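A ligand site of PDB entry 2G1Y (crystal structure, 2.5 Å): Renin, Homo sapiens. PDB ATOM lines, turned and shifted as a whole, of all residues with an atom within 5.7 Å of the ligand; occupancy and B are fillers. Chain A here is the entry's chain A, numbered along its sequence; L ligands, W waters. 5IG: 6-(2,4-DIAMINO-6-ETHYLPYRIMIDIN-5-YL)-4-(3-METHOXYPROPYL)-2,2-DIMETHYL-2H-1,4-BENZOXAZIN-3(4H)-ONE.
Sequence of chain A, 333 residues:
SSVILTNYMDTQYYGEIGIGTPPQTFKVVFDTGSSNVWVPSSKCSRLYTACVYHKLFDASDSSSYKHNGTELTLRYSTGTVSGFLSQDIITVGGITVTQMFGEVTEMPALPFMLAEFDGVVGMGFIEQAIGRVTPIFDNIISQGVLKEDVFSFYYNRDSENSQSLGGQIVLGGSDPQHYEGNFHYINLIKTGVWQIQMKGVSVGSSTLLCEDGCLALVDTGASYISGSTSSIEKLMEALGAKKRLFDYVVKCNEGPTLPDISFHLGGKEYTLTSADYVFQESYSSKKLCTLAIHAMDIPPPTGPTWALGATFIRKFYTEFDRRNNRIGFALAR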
ATOM      1  N   THR A  11       1.046  -5.008 -14.528  1.00  0.00           N
ATOM      2  CA  THR A  11       1.275  -3.584 -14.639  1.00  0.00           C
ATOM      3  C   THR A  11       0.979  -3.014 -16.015  1.00  0.00           C
ATOM      4  O   THR A  11       0.854  -1.796 -16.173  1.00  0.00           O
ATOM      5  CB  THR A  11       2.717  -3.238 -14.278  1.00  0.00           C
ATOM      6  OG1 THR A  11       3.615  -3.913 -15.175  1.00  0.00           O
ATOM      7  CG2 THR A  11       3.029  -3.656 -12.853  1.00  0.00           C
ATOM      8  N   GLN A  12       0.845  -3.883 -17.013  1.00  0.00           N
ATOM      9  CA  GLN A  12       0.557  -3.431 -18.368  1.00  0.00           C
ATOM     10  C   GLN A  12      -0.527  -4.272 -19.045  1.00  0.00           C
ATOM     11  O   GLN A  12      -0.390  -5.488 -19.164  1.00  0.00           O
ATOM     12  CB  GLN A  12       1.836  -3.485 -19.218  1.00  0.00           C
ATOM     13  CG  GLN A  12       2.920  -2.514 -18.763  1.00  0.00           C
ATOM     14  CD  GLN A  12       4.212  -2.670 -19.536  1.00  0.00           C
ATOM     15  OE1 GLN A  12       4.205  -2.697 -20.766  1.00  0.00           O
ATOM     16  NE2 GLN A  12       5.322  -2.779 -18.825  1.00  0.00           N
ATOM     17  N   TYR A  13      -1.605  -3.618 -19.463  1.00  0.00           N
ATOM     18  CA  TYR A  13      -2.685  -4.323 -20.140  1.00  0.00           C
ATOM     19  C   TYR A  13      -2.835  -3.680 -21.498  1.00  0.00           C
ATOM     20  O   TYR A  13      -2.976  -2.468 -21.600  1.00  0.00           O
ATOM     21  CB  TYR A  13      -3.998  -4.225 -19.347  1.00  0.00           C
ATOM     22  CG  TYR A  13      -3.991  -4.995 -18.035  1.00  0.00           C
ATOM     23  CD1 TYR A  13      -3.461  -4.442 -16.886  1.00  0.00           C
ATOM     24  CD2 TYR A  13      -4.512  -6.283 -17.966  1.00  0.00           C
ATOM     25  CE1 TYR A  13      -3.451  -5.151 -15.690  1.00  0.00           C
ATOM     26  CE2 TYR A  13      -4.509  -6.999 -16.779  1.00  0.00           C
ATOM     27  CZ  TYR A  13      -3.971  -6.422 -15.645  1.00  0.00           C
ATOM     28  OH  TYR A  13      -3.976  -7.111 -14.445  1.00  0.00           O
ATOM     29  N   VAL A  29      -2.505   0.319 -25.161  1.00  0.00           N
ATOM     30  CA  VAL A  29      -3.214   0.324 -23.900  1.00  0.00           C
ATOM     31  C   VAL A  29      -4.475   1.161 -24.131  1.00  0.00           C
ATOM     32  O   VAL A  29      -4.406   2.226 -24.746  1.00  0.00           O
ATOM     33  CB  VAL A  29      -2.409   0.996 -22.774  1.00  0.00           C
ATOM     34  CG1 VAL A  29      -3.239   1.049 -21.512  1.00  0.00           C
ATOM     35  CG2 VAL A  29      -1.129   0.243 -22.542  1.00  0.00           C
ATOM     36  N   ASP A  31      -6.646   3.497 -22.631  1.00  0.00           N
ATOM     37  CA  ASP A  31      -6.490   4.419 -21.517  1.00  0.00           C
ATOM     38  C   ASP A  31      -7.613   5.423 -21.266  1.00  0.00           C
ATOM     39  O   ASP A  31      -7.796   6.364 -22.034  1.00  0.00           O
ATOM     40  CB  ASP A  31      -5.171   5.154 -21.745  1.00  0.00           C
ATOM     41  CG  ASP A  31      -4.914   6.247 -20.757  1.00  0.00           C
ATOM     42  OD1 ASP A  31      -4.131   7.152 -21.108  1.00  0.00           O
ATOM     43  OD2 ASP A  31      -5.445   6.202 -19.633  1.00  0.00           O
ATOM     44  N   THR A  32      -8.352   5.224 -20.177  1.00  0.00           N
ATOM     45  CA  THR A  32      -9.435   6.155 -19.841  1.00  0.00           C
ATOM     46  C   THR A  32      -8.839   7.405 -19.208  1.00  0.00           C
ATOM     47  O   THR A  32      -9.561   8.326 -18.868  1.00  0.00           O
ATOM     48  CB  THR A  32     -10.458   5.541 -18.859  1.00  0.00           C
ATOM     49  OG1 THR A  32      -9.794   5.067 -17.685  1.00  0.00           O
ATOM     50  CG2 THR A  32     -11.210   4.399 -19.529  1.00  0.00           C
ATOM     51  N   GLY A  33      -7.523   7.415 -19.043  1.00  0.00           N
ATOM     52  CA  GLY A  33      -6.845   8.556 -18.457  1.00  0.00           C
ATOM     53  C   GLY A  33      -6.282   9.553 -19.459  1.00  0.00           C
ATOM     54  O   GLY A  33      -5.569  10.481 -19.081  1.00  0.00           O
ATOM     55  N   SER A  34      -6.574   9.353 -20.738  1.00  0.00           N
ATOM     56  CA  SER A  34      -6.107  10.265 -21.781  1.00  0.00           C
ATOM     57  C   SER A  34      -7.108  10.203 -22.928  1.00  0.00           C
ATOM     58  O   SER A  34      -8.018   9.363 -22.917  1.00  0.00           O
ATOM     59  CB  SER A  34      -4.684   9.928 -22.246  1.00  0.00           C
ATOM     60  OG  SER A  34      -4.606   8.659 -22.879  1.00  0.00           O
ATOM     61  N   TYR A  76       2.029  12.264 -19.938  1.00  0.00           N
ATOM     62  CA  TYR A  76       1.441  11.298 -19.017  1.00  0.00           C
ATOM     63  C   TYR A  76       2.184  11.458 -17.686  1.00  0.00           C
ATOM     64  O   TYR A  76       3.267  12.060 -17.636  1.00  0.00           O
ATOM     65  CB  TYR A  76       1.588   9.869 -19.544  1.00  0.00           C
ATOM     66  CG  TYR A  76       0.967   9.646 -20.894  1.00  0.00           C
ATOM     67  CD1 TYR A  76       1.742   9.665 -22.044  1.00  0.00           C
ATOM     68  CD2 TYR A  76      -0.402   9.432 -21.042  1.00  0.00           C
ATOM     69  CE1 TYR A  76       1.179   9.491 -23.299  1.00  0.00           C
ATOM     70  CE2 TYR A  76      -0.978   9.258 -22.297  1.00  0.00           C
ATOM     71  CZ  TYR A  76      -0.170   9.282 -23.423  1.00  0.00           C
ATOM     72  OH  TYR A  76      -0.711   9.097 -24.672  1.00  0.00           O
ATOM     73  N   SER A  77       1.609  10.929 -16.619  1.00  0.00           N
ATOM     74  CA  SER A  77       2.205  11.036 -15.300  1.00  0.00           C
ATOM     75  C   SER A  77       3.594  10.427 -15.209  1.00  0.00           C
ATOM     76  O   SER A  77       4.390  10.783 -14.343  1.00  0.00           O
ATOM     77  CB  SER A  77       1.301  10.379 -14.259  1.00  0.00           C
ATOM     78  OG  SER A  77       1.144   8.996 -14.529  1.00  0.00           O
ATOM     79  N   THR A  78       3.903   9.508 -16.121  1.00  0.00           N
ATOM     80  CA  THR A  78       5.189   8.864 -16.065  1.00  0.00           C
ATOM     81  C   THR A  78       6.024   8.945 -17.327  1.00  0.00           C
ATOM     82  O   THR A  78       7.028   8.255 -17.448  1.00  0.00           O
ATOM     83  CB  THR A  78       5.012   7.394 -15.693  1.00  0.00           C
ATOM     84  OG1 THR A  78       4.075   6.793 -16.592  1.00  0.00           O
ATOM     85  CG2 THR A  78       4.490   7.294 -14.283  1.00  0.00           C
ATOM     86  N   GLY A  79       5.623   9.808 -18.257  1.00  0.00           N
ATOM     87  CA  GLY A  79       6.391   9.928 -19.475  1.00  0.00           C
ATOM     88  C   GLY A  79       5.726  10.791 -20.517  1.00  0.00           C
ATOM     89  O   GLY A  79       4.510  11.005 -20.502  1.00  0.00           O
ATOM     90  N   PRO A 111      10.309   5.997 -19.886  1.00  0.00           N
ATOM     91  CA  PRO A 111       9.994   4.591 -19.619  1.00  0.00           C
ATOM     92  C   PRO A 111       9.699   3.658 -20.787  1.00  0.00           C
ATOM     93  O   PRO A 111       9.631   2.447 -20.598  1.00  0.00           O
ATOM     94  CB  PRO A 111       8.756   4.718 -18.764  1.00  0.00           C
ATOM     95  CG  PRO A 111       7.978   5.754 -19.575  1.00  0.00           C
ATOM     96  CD  PRO A 111       9.075   6.797 -19.898  1.00  0.00           C
ATOM     97  N   PHE A 112       9.538   4.179 -21.995  1.00  0.00           N
ATOM     98  CA  PHE A 112       9.117   3.314 -23.083  1.00  0.00           C
ATOM     99  C   PHE A 112       9.911   2.085 -23.465  1.00  0.00           C
ATOM    100  O   PHE A 112       9.380   1.195 -24.118  1.00  0.00           O
ATOM    101  CB  PHE A 112       8.765   4.171 -24.297  1.00  0.00           C
ATOM    102  CG  PHE A 112       7.669   5.141 -23.996  1.00  0.00           C
ATOM    103  CD1 PHE A 112       7.953   6.458 -23.694  1.00  0.00           C
ATOM    104  CD2 PHE A 112       6.364   4.698 -23.894  1.00  0.00           C
ATOM    105  CE1 PHE A 112       6.953   7.320 -23.285  1.00  0.00           C
ATOM    106  CE2 PHE A 112       5.356   5.559 -23.479  1.00  0.00           C
ATOM    107  CZ  PHE A 112       5.655   6.876 -23.177  1.00  0.00           C
ATOM    108  N   LEU A 114      10.652   0.082 -21.389  1.00  0.00           N
ATOM    109  CA  LEU A 114      10.058  -0.892 -20.478  1.00  0.00           C
ATOM    110  C   LEU A 114       8.607  -1.185 -20.804  1.00  0.00           C
ATOM    111  O   LEU A 114       7.952  -1.917 -20.073  1.00  0.00           O
ATOM    112  CB  LEU A 114      10.152  -0.389 -19.038  1.00  0.00           C
ATOM    113  CG  LEU A 114      11.567  -0.128 -18.517  1.00  0.00           C
ATOM    114  CD1 LEU A 114      11.484   0.455 -17.128  1.00  0.00           C
ATOM    115  CD2 LEU A 114      12.373  -1.415 -18.518  1.00  0.00           C
ATOM    116  N   ALA A 115       8.092  -0.616 -21.889  1.00  0.00           N
ATOM    117  CA  ALA A 115       6.713  -0.867 -22.289  1.00  0.00           C
ATOM    118  C   ALA A 115       6.596  -2.069 -23.198  1.00  0.00           C
ATOM    119  O   ALA A 115       7.317  -2.197 -24.192  1.00  0.00           O
ATOM    120  CB  ALA A 115       6.154   0.347 -23.000  1.00  0.00           C
ATOM    121  N   GLU A 116       5.687  -2.977 -22.853  1.00  0.00           N
ATOM    122  CA  GLU A 116       5.452  -4.155 -23.673  1.00  0.00           C
ATOM    123  C   GLU A 116       4.567  -3.714 -24.828  1.00  0.00           C
ATOM    124  O   GLU A 116       4.551  -4.347 -25.883  1.00  0.00           O
ATOM    125  CB  GLU A 116       4.730  -5.232 -22.860  1.00  0.00           C
ATOM    126  CG  GLU A 116       5.660  -6.271 -22.293  1.00  0.00           C
ATOM    127  CD  GLU A 116       5.920  -7.400 -23.277  1.00  0.00           C
ATOM    128  OE1 GLU A 116       6.110  -7.097 -24.478  1.00  0.00           O
ATOM    129  OE2 GLU A 116       5.954  -8.579 -22.842  1.00  0.00           O
ATOM    130  N   PHE A 117       3.848  -2.611 -24.630  1.00  0.00           N
ATOM    131  CA  PHE A 117       2.963  -2.080 -25.652  1.00  0.00           C
ATOM    132  C   PHE A 117       3.679  -1.118 -26.584  1.00  0.00           C
ATOM    133  O   PHE A 117       4.752  -0.623 -26.285  1.00  0.00           O
ATOM    134  CB  PHE A 117       1.772  -1.378 -25.016  1.00  0.00           C
ATOM    135  CG  PHE A 117       2.151  -0.273 -24.056  1.00  0.00           C
ATOM    136  CD1 PHE A 117       2.401  -0.555 -22.722  1.00  0.00           C
ATOM    137  CD2 PHE A 117       2.235   1.047 -24.500  1.00  0.00           C
ATOM    138  CE1 PHE A 117       2.721   0.474 -21.836  1.00  0.00           C
ATOM    139  CE2 PHE A 117       2.556   2.067 -23.617  1.00  0.00           C
ATOM    140  CZ  PHE A 117       2.791   1.785 -22.284  1.00  0.00           C
ATOM    141  N   GLY A 119       1.687   1.517 -28.388  1.00  0.00           N
ATOM    142  CA  GLY A 119       1.043   2.806 -28.218  1.00  0.00           C
ATOM    143  C   GLY A 119      -0.141   2.896 -27.297  1.00  0.00           C
ATOM    144  O   GLY A 119      -0.394   2.026 -26.462  1.00  0.00           O
ATOM    145  N   VAL A 120      -0.899   3.983 -27.471  1.00  0.00           N
ATOM    146  CA  VAL A 120      -2.061   4.233 -26.646  1.00  0.00           C
ATOM    147  C   VAL A 120      -3.310   4.680 -27.397  1.00  0.00           C
ATOM    148  O   VAL A 120      -3.242   5.479 -28.339  1.00  0.00           O
ATOM    149  CB  VAL A 120      -1.736   5.329 -25.581  1.00  0.00           C
ATOM    150  CG1 VAL A 120      -2.902   5.478 -24.607  1.00  0.00           C
ATOM    151  CG2 VAL A 120      -0.423   4.991 -24.879  1.00  0.00           C
ATOM    152  N   TYR A 155      -9.859  -6.533 -16.122  1.00  0.00           N
ATOM    153  CA  TYR A 155      -8.418  -6.713 -15.966  1.00  0.00           C
ATOM    154  C   TYR A 155      -8.263  -7.928 -15.067  1.00  0.00           C
ATOM    155  O   TYR A 155      -8.608  -7.868 -13.886  1.00  0.00           O
ATOM    156  CB  TYR A 155      -7.759  -5.513 -15.292  1.00  0.00           C
ATOM    157  CG  TYR A 155      -7.421  -4.395 -16.234  1.00  0.00           C
ATOM    158  CD1 TYR A 155      -6.851  -3.214 -15.774  1.00  0.00           C
ATOM    159  CD2 TYR A 155      -7.661  -4.512 -17.585  1.00  0.00           C
ATOM    160  CE1 TYR A 155      -6.529  -2.189 -16.638  1.00  0.00           C
ATOM    161  CE2 TYR A 155      -7.346  -3.494 -18.459  1.00  0.00           C
ATOM    162  CZ  TYR A 155      -6.784  -2.329 -17.981  1.00  0.00           C
ATOM    163  OH  TYR A 155      -6.467  -1.331 -18.861  1.00  0.00           O
ATOM    164  N   ASP A 219      -8.685   5.469 -13.932  1.00  0.00           N
ATOM    165  CA  ASP A 219      -7.719   5.352 -15.015  1.00  0.00           C
ATOM    166  C   ASP A 219      -7.337   3.936 -15.441  1.00  0.00           C
ATOM    167  O   ASP A 219      -6.576   3.272 -14.752  1.00  0.00           O
ATOM    168  CB  ASP A 219      -6.473   6.134 -14.604  1.00  0.00           C
ATOM    169  CG  ASP A 219      -5.585   6.482 -15.772  1.00  0.00           C
ATOM    170  OD1 ASP A 219      -4.547   7.116 -15.533  1.00  0.00           O
ATOM    171  OD2 ASP A 219      -5.936   6.141 -16.916  1.00  0.00           O
ATOM    172  N   THR A 220      -7.856   3.484 -16.578  1.00  0.00           N
ATOM    173  CA  THR A 220      -7.536   2.144 -17.067  1.00  0.00           C
ATOM    174  C   THR A 220      -6.122   2.077 -17.614  1.00  0.00           C
ATOM    175  O   THR A 220      -5.600   0.986 -17.845  1.00  0.00           O
ATOM    176  CB  THR A 220      -8.466   1.712 -18.214  1.00  0.00           C
ATOM    177  OG1 THR A 220      -8.322   2.618 -19.315  1.00  0.00           O
ATOM    178  CG2 THR A 220      -9.902   1.667 -17.756  1.00  0.00           C
ATOM    179  N   GLY A 221      -5.501   3.235 -17.809  1.00  0.00           N
ATOM    180  CA  GLY A 221      -4.160   3.270 -18.361  1.00  0.00           C
ATOM    181  C   GLY A 221      -3.085   3.424 -17.318  1.00  0.00           C
ATOM    182  O   GLY A 221      -1.913   3.658 -17.663  1.00  0.00           O
ATOM    183  N   ALA A 222      -3.451   3.294 -16.049  1.00  0.00           N
ATOM    184  CA  ALA A 222      -2.505   3.412 -14.963  1.00  0.00           C
ATOM    185  C   ALA A 222      -2.323   2.057 -14.275  1.00  0.00           C
ATOM    186  O   ALA A 222      -3.287   1.317 -14.063  1.00  0.00           O
ATOM    187  CB  ALA A 222      -2.983   4.436 -13.963  1.00  0.00           C
ATOM    188  N   SER A 223      -1.079   1.726 -13.925  1.00  0.00           N
ATOM    189  CA  SER A 223      -0.798   0.450 -13.286  1.00  0.00           C
ATOM    190  C   SER A 223      -1.299   0.329 -11.874  1.00  0.00           C
ATOM    191  O   SER A 223      -1.607  -0.761 -11.429  1.00  0.00           O
ATOM    192  CB  SER A 223       0.707   0.181 -13.253  1.00  0.00           C
ATOM    193  OG  SER A 223       1.243   0.096 -14.550  1.00  0.00           O
ATOM    194  N   MET A 296       1.468   9.739  -6.442  1.00  0.00           N
ATOM    195  CA  MET A 296       1.499  10.395  -7.745  1.00  0.00           C
ATOM    196  C   MET A 296       0.620  11.633  -7.686  1.00  0.00           C
ATOM    197  O   MET A 296      -0.592  11.537  -7.592  1.00  0.00           O
ATOM    198  CB  MET A 296       0.981   9.430  -8.820  1.00  0.00           C
ATOM    199  CG  MET A 296       1.250   9.860 -10.262  1.00  0.00           C
ATOM    200  SD  MET A 296       2.017   8.511 -11.248  1.00  0.00           S
ATOM    201  CE  MET A 296       0.557   7.541 -11.834  1.00  0.00           C
ATOM    202  N   ALA A 310      -5.196  -0.210 -12.480  1.00  0.00           N
ATOM    203  CA  ALA A 310      -5.282  -1.659 -12.568  1.00  0.00           C
ATOM    204  C   ALA A 310      -5.405  -2.377 -11.233  1.00  0.00           C
ATOM    205  O   ALA A 310      -6.045  -3.425 -11.148  1.00  0.00           O
ATOM    206  CB  ALA A 310      -4.088  -2.202 -13.338  1.00  0.00           C
HETATM  207  C1  5IG L   1      -0.250   6.797 -17.701  1.00  0.00           C
HETATM  208  N1  5IG L   1      -1.422   7.416 -17.452  1.00  0.00           N
HETATM  209  C2  5IG L   1      -2.326   7.396 -18.430  1.00  0.00           C
HETATM  210  N2  5IG L   1      -2.138   6.807 -19.626  1.00  0.00           N
HETATM  211  C3  5IG L   1      -0.958   6.183 -19.898  1.00  0.00           C
HETATM  212  C4  5IG L   1       0.046   6.144 -18.917  1.00  0.00           C
HETATM  213  N3  5IG L   1       0.645   6.830 -16.697  1.00  0.00           N
HETATM  214  N4  5IG L   1      -3.501   7.986 -18.226  1.00  0.00           N
HETATM  215  C6  5IG L   1      -0.825   5.538 -21.279  1.00  0.00           C
HETATM  216  C7  5IG L   1       2.485   6.014 -19.725  1.00  0.00           C
HETATM  217  C8  5IG L   1       3.667   5.238 -19.810  1.00  0.00           C
HETATM  218  C9  5IG L   1       3.719   3.934 -19.254  1.00  0.00           C
HETATM  219  C10 5IG L   1       2.569   3.375 -18.613  1.00  0.00           C
HETATM  220  C11 5IG L   1       1.417   4.163 -18.568  1.00  0.00           C
HETATM  221  C12 5IG L   1       1.350   5.459 -19.098  1.00  0.00           C
HETATM  222  O3  5IG L   1       4.915   3.254 -19.386  1.00  0.00           O
HETATM  223  C14 5IG L   1       5.104   2.056 -18.628  1.00  0.00           C
HETATM  224  C15 5IG L   1       3.797   1.344 -18.056  1.00  0.00           C
HETATM  225  N5  5IG L   1       2.613   2.082 -18.061  1.00  0.00           N
HETATM  226  C16 5IG L   1       1.424   1.422 -17.435  1.00  0.00           C
HETATM  227  C17 5IG L   1       0.508   0.648 -18.423  1.00  0.00           C
HETATM  228  C18 5IG L   1      -0.935   0.507 -17.911  1.00  0.00           C
HETATM  229  O1  5IG L   1      -1.619  -0.526 -18.593  1.00  0.00           O
HETATM  230  C19 5IG L   1      -2.963  -0.739 -18.190  1.00  0.00           C
HETATM  231  C21 5IG L   1       6.004   2.398 -17.418  1.00  0.00           C
HETATM  232  C20 5IG L   1       5.854   1.123 -19.585  1.00  0.00           C
HETATM  233  O4  5IG L   1       3.892   0.222 -17.596  1.00  0.00           O
HETATM  234  C5  5IG L   1      -1.302   4.094 -21.315  1.00  0.00           C
HETATM  235  O   HOH W   1       5.253  -1.623 -16.157  1.00  0.00           O
HETATM  236  O   HOH W   2      -1.415  10.062 -16.969  1.00  0.00           O
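O of Thr 11 touches C17 of the ligand (3.3 Å). Gln 12 touches the ligand (CG to O4, 3.1 Å). Val 29 touches the ligand (CB to C5, 3.6 Å). Tyr 76 touches the ligand (CD2 to N2, 3.5 Å). Pro 111 touches the ligand. Leu 114 touches the ligand (O to C20, 3.7 Å). Ala 115 touches the ligand. Phe 117 touches the ligand. CG2 of Val 120 touches C6 of the ligand, at 3.7 Å. OH of Tyr 155 touches C19 of the ligand, 3.6 Å away. O of Thr 220 touches C19 of the ligand, at 3.2 Å. Gly 221 touches the ligand. Ser 223 touches the ligand (OG to C16, 3.2 Å). Hydrophobic or aromatic side chains within 4 Å of the ligand: Tyr 13, Val 29, Tyr 76, Pro 111, Ala 115, Phe 117 and Val 120. Of the 28 residues printed, 19 come within 4 Å of the ligand.
OD2 of Asp 31 lies close to N of Gly 221. OD1 of Asp 31 lies close to N of Ser 34, at 3.3 Å. The backbone NH (N) of Gly 33 lies within hydrogen-bond range of the side-chain carboxylate (OD2) of Asp 219, 2.9 Å away. NE2 of Gln 12 sits at hydrogen-bond distance from O of Leu 114 (3.0 Å). The side-chain amide oxygen (OE1) of Gln 12 sits at hydrogen-bond distance from the backbone NH (N) of Glu 116, 2.6 Å away. The backbone NH (N) of Thr 220 lies within hydrogen-bond range of the side-chain hydroxyl (OG1) of Thr 32 (2.7 Å). OG of Ser 223 is in hydrogen-bond range of O of Thr 11. N of Val 29 lies within hydrogen-bond range of O of Gly 119, at 3.0 Å.
The side-chain carboxylate (OD1) of Asp 31 lies within hydrogen-bond range of a nitrogen (N2) of the ligand (2.5 Å). N4 of the ligand sits at hydrogen-bond distance from OD1 of Asp 219 (3.0 Å). The side-chain hydroxyl of Ser 77 lies within hydrogen-bond range of a nitrogen (N3) of the ligand (3.1 Å). An oxygen (O1) of the ligand lies within hydrogen-bond range of the backbone NH (N) of Tyr 13 (3.2 Å). N4 of the ligand lies within hydrogen-bond range of O of Gly 33 (3.4 Å). OG1 of Thr 78 lies within hydrogen-bond range of N3 of the ligand, 3.4 Å away.
Water W2 bridges N1 of the ligand (2.7 Å) and N of Ser 77 (3.2 Å). Water W1 lies within hydrogen-bond range of O4 of the ligand, NE2 of Gln 12 and OG1 of Thr 11.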
